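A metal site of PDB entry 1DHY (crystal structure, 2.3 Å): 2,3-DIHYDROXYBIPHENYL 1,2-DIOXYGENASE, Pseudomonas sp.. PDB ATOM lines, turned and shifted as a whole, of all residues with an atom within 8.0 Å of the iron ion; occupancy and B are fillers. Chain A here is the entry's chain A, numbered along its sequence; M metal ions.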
ATOM      1  N   HIS A 145     -21.998  -2.976 -27.690  1.00  0.00           N
ATOM      2  CA  HIS A 145     -20.662  -2.390 -27.561  1.00  0.00           C
ATOM      3  C   HIS A 145     -20.698  -1.204 -26.593  1.00  0.00           C
ATOM      4  O   HIS A 145     -21.778  -0.731 -26.282  1.00  0.00           O
ATOM      5  CB  HIS A 145     -20.108  -1.933 -28.908  1.00  0.00           C
ATOM      6  CG  HIS A 145     -20.768  -0.708 -29.468  1.00  0.00           C
ATOM      7  ND1 HIS A 145     -21.510  -0.725 -30.628  1.00  0.00           N
ATOM      8  CD2 HIS A 145     -20.790   0.578 -29.040  1.00  0.00           C
ATOM      9  CE1 HIS A 145     -21.957   0.483 -30.893  1.00  0.00           C
ATOM     10  NE2 HIS A 145     -21.536   1.300 -29.938  1.00  0.00           N
ATOM     11  N   PHE A 146     -19.541  -0.781 -26.090  1.00  0.00           N
ATOM     12  CA  PHE A 146     -19.481   0.403 -25.217  1.00  0.00           C
ATOM     13  C   PHE A 146     -18.247   1.230 -25.489  1.00  0.00           C
ATOM     14  O   PHE A 146     -17.325   0.747 -26.156  1.00  0.00           O
ATOM     15  CB  PHE A 146     -19.612   0.076 -23.722  1.00  0.00           C
ATOM     16  CG  PHE A 146     -18.530  -0.820 -23.168  1.00  0.00           C
ATOM     17  CD1 PHE A 146     -18.691  -2.209 -23.185  1.00  0.00           C
ATOM     18  CD2 PHE A 146     -17.421  -0.275 -22.518  1.00  0.00           C
ATOM     19  CE1 PHE A 146     -17.761  -3.038 -22.553  1.00  0.00           C
ATOM     20  CE2 PHE A 146     -16.480  -1.096 -21.883  1.00  0.00           C
ATOM     21  CZ  PHE A 146     -16.651  -2.472 -21.897  1.00  0.00           C
ATOM     22  N   VAL A 147     -18.311   2.497 -25.127  1.00  0.00           N
ATOM     23  CA  VAL A 147     -17.208   3.431 -25.302  1.00  0.00           C
ATOM     24  C   VAL A 147     -16.577   3.667 -23.956  1.00  0.00           C
ATOM     25  O   VAL A 147     -17.185   4.251 -23.064  1.00  0.00           O
ATOM     26  CB  VAL A 147     -17.681   4.747 -25.936  1.00  0.00           C
ATOM     27  CG1 VAL A 147     -16.605   5.816 -25.903  1.00  0.00           C
ATOM     28  CG2 VAL A 147     -18.068   4.484 -27.392  1.00  0.00           C
ATOM     29  N   PHE A 186     -11.812   2.295 -32.442  1.00  0.00           N
ATOM     30  CA  PHE A 186     -12.844   1.290 -32.388  1.00  0.00           C
ATOM     31  C   PHE A 186     -12.234  -0.065 -32.617  1.00  0.00           C
ATOM     32  O   PHE A 186     -11.482  -0.257 -33.559  1.00  0.00           O
ATOM     33  CB  PHE A 186     -13.937   1.650 -33.419  1.00  0.00           C
ATOM     34  CG  PHE A 186     -14.505   3.060 -33.232  1.00  0.00           C
ATOM     35  CD1 PHE A 186     -13.782   4.186 -33.636  1.00  0.00           C
ATOM     36  CD2 PHE A 186     -15.740   3.260 -32.609  1.00  0.00           C
ATOM     37  CE1 PHE A 186     -14.273   5.492 -33.425  1.00  0.00           C
ATOM     38  CE2 PHE A 186     -16.237   4.559 -32.387  1.00  0.00           C
ATOM     39  CZ  PHE A 186     -15.502   5.680 -32.796  1.00  0.00           C
ATOM     40  N   HIS A 194     -17.562  -2.957 -33.986  1.00  0.00           N
ATOM     41  CA  HIS A 194     -16.814  -2.732 -32.758  1.00  0.00           C
ATOM     42  C   HIS A 194     -17.531  -3.213 -31.532  1.00  0.00           C
ATOM     43  O   HIS A 194     -18.775  -3.186 -31.483  1.00  0.00           O
ATOM     44  CB  HIS A 194     -16.306  -1.281 -32.636  1.00  0.00           C
ATOM     45  CG  HIS A 194     -17.351  -0.247 -32.319  1.00  0.00           C
ATOM     46  ND1 HIS A 194     -18.199   0.275 -33.268  1.00  0.00           N
ATOM     47  CD2 HIS A 194     -17.583   0.453 -31.184  1.00  0.00           C
ATOM     48  CE1 HIS A 194     -18.900   1.261 -32.742  1.00  0.00           C
ATOM     49  NE2 HIS A 194     -18.550   1.389 -31.474  1.00  0.00           N
ATOM     50  N   ALA A 197     -14.799   0.731 -27.816  1.00  0.00           N
ATOM     51  CA  ALA A 197     -14.190   1.901 -28.419  1.00  0.00           C
ATOM     52  C   ALA A 197     -13.467   2.535 -27.256  1.00  0.00           C
ATOM     53  O   ALA A 197     -13.991   2.538 -26.143  1.00  0.00           O
ATOM     54  CB  ALA A 197     -15.229   2.867 -28.987  1.00  0.00           C
ATOM     55  N   HIS A 208     -18.926   5.972 -21.830  1.00  0.00           N
ATOM     56  CA  HIS A 208     -19.702   7.108 -22.299  1.00  0.00           C
ATOM     57  C   HIS A 208     -21.101   6.619 -22.667  1.00  0.00           C
ATOM     58  O   HIS A 208     -22.079   7.345 -22.507  1.00  0.00           O
ATOM     59  CB  HIS A 208     -19.044   7.734 -23.520  1.00  0.00           C
ATOM     60  CG  HIS A 208     -19.891   8.749 -24.216  1.00  0.00           C
ATOM     61  ND1 HIS A 208     -20.831   8.413 -25.167  1.00  0.00           N
ATOM     62  CD2 HIS A 208     -19.954  10.094 -24.095  1.00  0.00           C
ATOM     63  CE1 HIS A 208     -21.425   9.510 -25.612  1.00  0.00           C
ATOM     64  NE2 HIS A 208     -20.916  10.547 -24.970  1.00  0.00           N
ATOM     65  N   HIS A 209     -21.191   5.419 -23.227  1.00  0.00           N
ATOM     66  CA  HIS A 209     -22.479   4.853 -23.608  1.00  0.00           C
ATOM     67  C   HIS A 209     -22.363   3.396 -24.010  1.00  0.00           C
ATOM     68  O   HIS A 209     -21.263   2.946 -24.330  1.00  0.00           O
ATOM     69  CB  HIS A 209     -23.052   5.626 -24.797  1.00  0.00           C
ATOM     70  CG  HIS A 209     -22.399   5.300 -26.115  1.00  0.00           C
ATOM     71  ND1 HIS A 209     -21.494   6.150 -26.718  1.00  0.00           N
ATOM     72  CD2 HIS A 209     -22.589   4.290 -26.985  1.00  0.00           C
ATOM     73  CE1 HIS A 209     -21.174   5.677 -27.914  1.00  0.00           C
ATOM     74  NE2 HIS A 209     -21.834   4.556 -28.105  1.00  0.00           N
ATOM     75  N   PHE A 210     -23.467   2.665 -23.956  1.00  0.00           N
ATOM     76  CA  PHE A 210     -23.531   1.271 -24.422  1.00  0.00           C
ATOM     77  C   PHE A 210     -24.593   1.266 -25.508  1.00  0.00           C
ATOM     78  O   PHE A 210     -25.426   2.156 -25.569  1.00  0.00           O
ATOM     79  CB  PHE A 210     -23.880   0.269 -23.335  1.00  0.00           C
ATOM     80  CG  PHE A 210     -25.216   0.463 -22.737  1.00  0.00           C
ATOM     81  CD1 PHE A 210     -25.465   1.525 -21.883  1.00  0.00           C
ATOM     82  CD2 PHE A 210     -26.213  -0.487 -22.937  1.00  0.00           C
ATOM     83  CE1 PHE A 210     -26.679   1.632 -21.204  1.00  0.00           C
ATOM     84  CE2 PHE A 210     -27.438  -0.400 -22.268  1.00  0.00           C
ATOM     85  CZ  PHE A 210     -27.672   0.661 -21.397  1.00  0.00           C
ATOM     86  N   MET A 211     -24.578   0.263 -26.358  1.00  0.00           N
ATOM     87  CA  MET A 211     -25.520   0.285 -27.450  1.00  0.00           C
ATOM     88  C   MET A 211     -26.170  -1.045 -27.670  1.00  0.00           C
ATOM     89  O   MET A 211     -25.500  -2.062 -27.582  1.00  0.00           O
ATOM     90  CB  MET A 211     -24.782   0.690 -28.713  1.00  0.00           C
ATOM     91  CG  MET A 211     -25.583   0.602 -29.976  1.00  0.00           C
ATOM     92  SD  MET A 211     -25.291  -0.907 -30.904  1.00  0.00           S
ATOM     93  CE  MET A 211     -26.077  -0.483 -32.498  1.00  0.00           C
ATOM     94  N   LEU A 212     -27.476  -1.017 -27.932  1.00  0.00           N
ATOM     95  CA  LEU A 212     -28.248  -2.226 -28.219  1.00  0.00           C
ATOM     96  C   LEU A 212     -28.683  -2.075 -29.683  1.00  0.00           C
ATOM     97  O   LEU A 212     -29.031  -0.973 -30.102  1.00  0.00           O
ATOM     98  CB  LEU A 212     -29.453  -2.324 -27.283  1.00  0.00           C
ATOM     99  CG  LEU A 212     -29.129  -2.416 -25.788  1.00  0.00           C
ATOM    100  CD1 LEU A 212     -30.371  -2.133 -24.980  1.00  0.00           C
ATOM    101  CD2 LEU A 212     -28.571  -3.782 -25.450  1.00  0.00           C
ATOM    102  N   HIS A 240     -23.820   6.573 -38.299  1.00  0.00           N
ATOM    103  CA  HIS A 240     -22.384   6.718 -38.167  1.00  0.00           C
ATOM    104  C   HIS A 240     -21.582   6.534 -39.445  1.00  0.00           C
ATOM    105  O   HIS A 240     -22.027   5.865 -40.372  1.00  0.00           O
ATOM    106  CB  HIS A 240     -21.860   5.810 -37.061  1.00  0.00           C
ATOM    107  CG  HIS A 240     -22.139   6.361 -35.693  1.00  0.00           C
ATOM    108  ND1 HIS A 240     -22.895   5.677 -34.759  1.00  0.00           N
ATOM    109  CD2 HIS A 240     -21.776   7.515 -35.116  1.00  0.00           C
ATOM    110  CE1 HIS A 240     -22.987   6.414 -33.669  1.00  0.00           C
ATOM    111  NE2 HIS A 240     -22.321   7.528 -33.848  1.00  0.00           N
ATOM    112  N   ASN A 242     -18.310   5.300 -39.599  1.00  0.00           N
ATOM    113  CA  ASN A 242     -17.543   4.082 -39.608  1.00  0.00           C
ATOM    114  C   ASN A 242     -18.261   2.779 -39.584  1.00  0.00           C
ATOM    115  O   ASN A 242     -17.879   1.904 -40.340  1.00  0.00           O
ATOM    116  CB  ASN A 242     -16.473   4.134 -38.541  1.00  0.00           C
ATOM    117  CG  ASN A 242     -17.022   4.208 -37.159  1.00  0.00           C
ATOM    118  OD1 ASN A 242     -18.238   4.220 -36.952  1.00  0.00           O
ATOM    119  ND2 ASN A 242     -16.130   4.194 -36.176  1.00  0.00           N
ATOM    120  N   ASP A 243     -19.228   2.580 -38.707  1.00  0.00           N
ATOM    121  CA  ASP A 243     -19.970   1.311 -38.713  1.00  0.00           C
ATOM    122  C   ASP A 243     -21.338   1.428 -39.398  1.00  0.00           C
ATOM    123  O   ASP A 243     -22.039   0.429 -39.560  1.00  0.00           O
ATOM    124  CB  ASP A 243     -20.147   0.722 -37.298  1.00  0.00           C
ATOM    125  CG  ASP A 243     -21.027   1.579 -36.385  1.00  0.00           C
ATOM    126  OD1 ASP A 243     -21.264   2.780 -36.700  1.00  0.00           O
ATOM    127  OD2 ASP A 243     -21.469   1.050 -35.351  1.00  0.00           O
ATOM    128  N   THR A 245     -24.133   2.522 -38.296  1.00  0.00           N
ATOM    129  CA  THR A 245     -25.280   2.203 -37.455  1.00  0.00           C
ATOM    130  C   THR A 245     -26.220   3.412 -37.565  1.00  0.00           C
ATOM    131  O   THR A 245     -25.750   4.553 -37.539  1.00  0.00           O
ATOM    132  CB  THR A 245     -24.852   2.050 -35.948  1.00  0.00           C
ATOM    133  OG1 THR A 245     -24.626   0.674 -35.623  1.00  0.00           O
ATOM    134  CG2 THR A 245     -25.925   2.576 -35.020  1.00  0.00           C
ATOM    135  N   SER A 247     -28.961   5.264 -35.566  1.00  0.00           N
ATOM    136  CA  SER A 247     -29.421   5.291 -34.181  1.00  0.00           C
ATOM    137  C   SER A 247     -29.682   6.683 -33.663  1.00  0.00           C
ATOM    138  O   SER A 247     -29.559   7.674 -34.369  1.00  0.00           O
ATOM    139  CB  SER A 247     -28.320   4.698 -33.337  1.00  0.00           C
ATOM    140  OG  SER A 247     -27.117   5.408 -33.601  1.00  0.00           O
ATOM    141  N   TYR A 249     -29.379   8.721 -29.463  1.00  0.00           N
ATOM    142  CA  TYR A 249     -28.838   8.528 -28.134  1.00  0.00           C
ATOM    143  C   TYR A 249     -29.802   9.093 -27.153  1.00  0.00           C
ATOM    144  O   TYR A 249     -30.494  10.054 -27.444  1.00  0.00           O
ATOM    145  CB  TYR A 249     -27.510   9.279 -27.975  1.00  0.00           C
ATOM    146  CG  TYR A 249     -26.363   8.661 -28.741  1.00  0.00           C
ATOM    147  CD1 TYR A 249     -26.251   8.856 -30.108  1.00  0.00           C
ATOM    148  CD2 TYR A 249     -25.386   7.926 -28.093  1.00  0.00           C
ATOM    149  CE1 TYR A 249     -25.221   8.323 -30.819  1.00  0.00           C
ATOM    150  CE2 TYR A 249     -24.346   7.392 -28.800  1.00  0.00           C
ATOM    151  CZ  TYR A 249     -24.271   7.607 -30.176  1.00  0.00           C
ATOM    152  OH  TYR A 249     -23.233   7.106 -30.937  1.00  0.00           O
ATOM    153  N   VAL A 259     -27.334   5.821 -23.621  1.00  0.00           N
ATOM    154  CA  VAL A 259     -27.642   4.626 -24.419  1.00  0.00           C
ATOM    155  C   VAL A 259     -27.748   5.042 -25.863  1.00  0.00           C
ATOM    156  O   VAL A 259     -28.082   6.186 -26.189  1.00  0.00           O
ATOM    157  CB  VAL A 259     -29.002   3.988 -24.191  1.00  0.00           C
ATOM    158  CG1 VAL A 259     -28.827   2.541 -23.811  1.00  0.00           C
ATOM    159  CG2 VAL A 259     -29.812   4.770 -23.221  1.00  0.00           C
ATOM    160  N   GLU A 260     -27.528   4.070 -26.731  1.00  0.00           N
ATOM    161  CA  GLU A 260     -27.634   4.248 -28.144  1.00  0.00           C
ATOM    162  C   GLU A 260     -28.480   3.054 -28.607  1.00  0.00           C
ATOM    163  O   GLU A 260     -28.189   1.904 -28.263  1.00  0.00           O
ATOM    164  CB  GLU A 260     -26.258   4.206 -28.778  1.00  0.00           C
ATOM    165  CG  GLU A 260     -26.323   4.381 -30.263  1.00  0.00           C
ATOM    166  CD  GLU A 260     -25.021   4.076 -30.965  1.00  0.00           C
ATOM    167  OE1 GLU A 260     -24.096   3.511 -30.339  1.00  0.00           O
ATOM    168  OE2 GLU A 260     -24.920   4.406 -32.163  1.00  0.00           O
ATOM    169  N   PHE A 261     -29.585   3.346 -29.294  1.00  0.00           N
ATOM    170  CA  PHE A 261     -30.491   2.319 -29.814  1.00  0.00           C
ATOM    171  C   PHE A 261     -30.266   2.448 -31.319  1.00  0.00           C
ATOM    172  O   PHE A 261     -30.441   3.516 -31.894  1.00  0.00           O
ATOM    173  CB  PHE A 261     -31.956   2.671 -29.451  1.00  0.00           C
ATOM    174  CG  PHE A 261     -32.885   1.468 -29.326  1.00  0.00           C
ATOM    175  CD1 PHE A 261     -33.044   0.821 -28.108  1.00  0.00           C
ATOM    176  CD2 PHE A 261     -33.607   1.001 -30.434  1.00  0.00           C
ATOM    177  CE1 PHE A 261     -33.908  -0.286 -27.983  1.00  0.00           C
ATOM    178  CE2 PHE A 261     -34.464  -0.099 -30.320  1.00  0.00           C
ATOM    179  CZ  PHE A 261     -34.611  -0.739 -29.100  1.00  0.00           C
ATOM    180  N   HIS A 285     -27.745  12.722 -36.277  1.00  0.00           N
ATOM    181  CA  HIS A 285     -27.138  12.804 -34.954  1.00  0.00           C
ATOM    182  C   HIS A 285     -26.997  14.196 -34.360  1.00  0.00           C
ATOM    183  O   HIS A 285     -26.146  14.414 -33.521  1.00  0.00           O
ATOM    184  CB  HIS A 285     -25.808  12.048 -34.916  1.00  0.00           C
ATOM    185  CG  HIS A 285     -25.957  10.562 -34.859  1.00  0.00           C
ATOM    186  ND1 HIS A 285     -27.104   9.951 -34.392  1.00  0.00           N
ATOM    187  CD2 HIS A 285     -25.105   9.554 -35.179  1.00  0.00           C
ATOM    188  CE1 HIS A 285     -26.953   8.637 -34.421  1.00  0.00           C
ATOM    189  NE2 HIS A 285     -25.752   8.364 -34.905  1.00  0.00           N
HETATM  190 FE    FE M   1     -21.697   3.617 -30.260  1.00  0.00          FE
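Tyr 249 touches the iron ion.
Of the 21 residues printed, 4 come within 4 Å of the iron ion.
OE2 of Glu 260 sits at hydrogen-bond distance from OG of Ser 247 (2.8 Å).
ND1 of His 209 sits at hydrogen-bond distance from ND1 of His 208 (2.8 Å).
The side-chain hydroxyl (OH) of Tyr 249 lies close to a ring nitrogen (NE2) of His 240 (3.1 Å).
A ring nitrogen (NE2) of His 145 sits close to a ring nitrogen (NE2) of His 194 (3.4 Å).
The backbone NH of Leu 212 sits at hydrogen-bond distance from the backbone carbonyl oxygen of Glu 260 (3.0 Å).
N of Glu 260 lies within hydrogen-bond range of O of Phe 210, 3.1 Å away.
The side-chain carboxylate of Glu 260 is in hydrogen-bond range of the side-chain hydroxyl of Tyr 249, 3.4 Å away.
The backbone carbonyl oxygen (O) of His 145 is in hydrogen-bond range of the backbone NH (N) of Met 211.
The iron ion is bound by NE2 of His 145, NE2 of His 209 and OE1 of Glu 260.
The iron ion has three donor atoms within binding distance.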
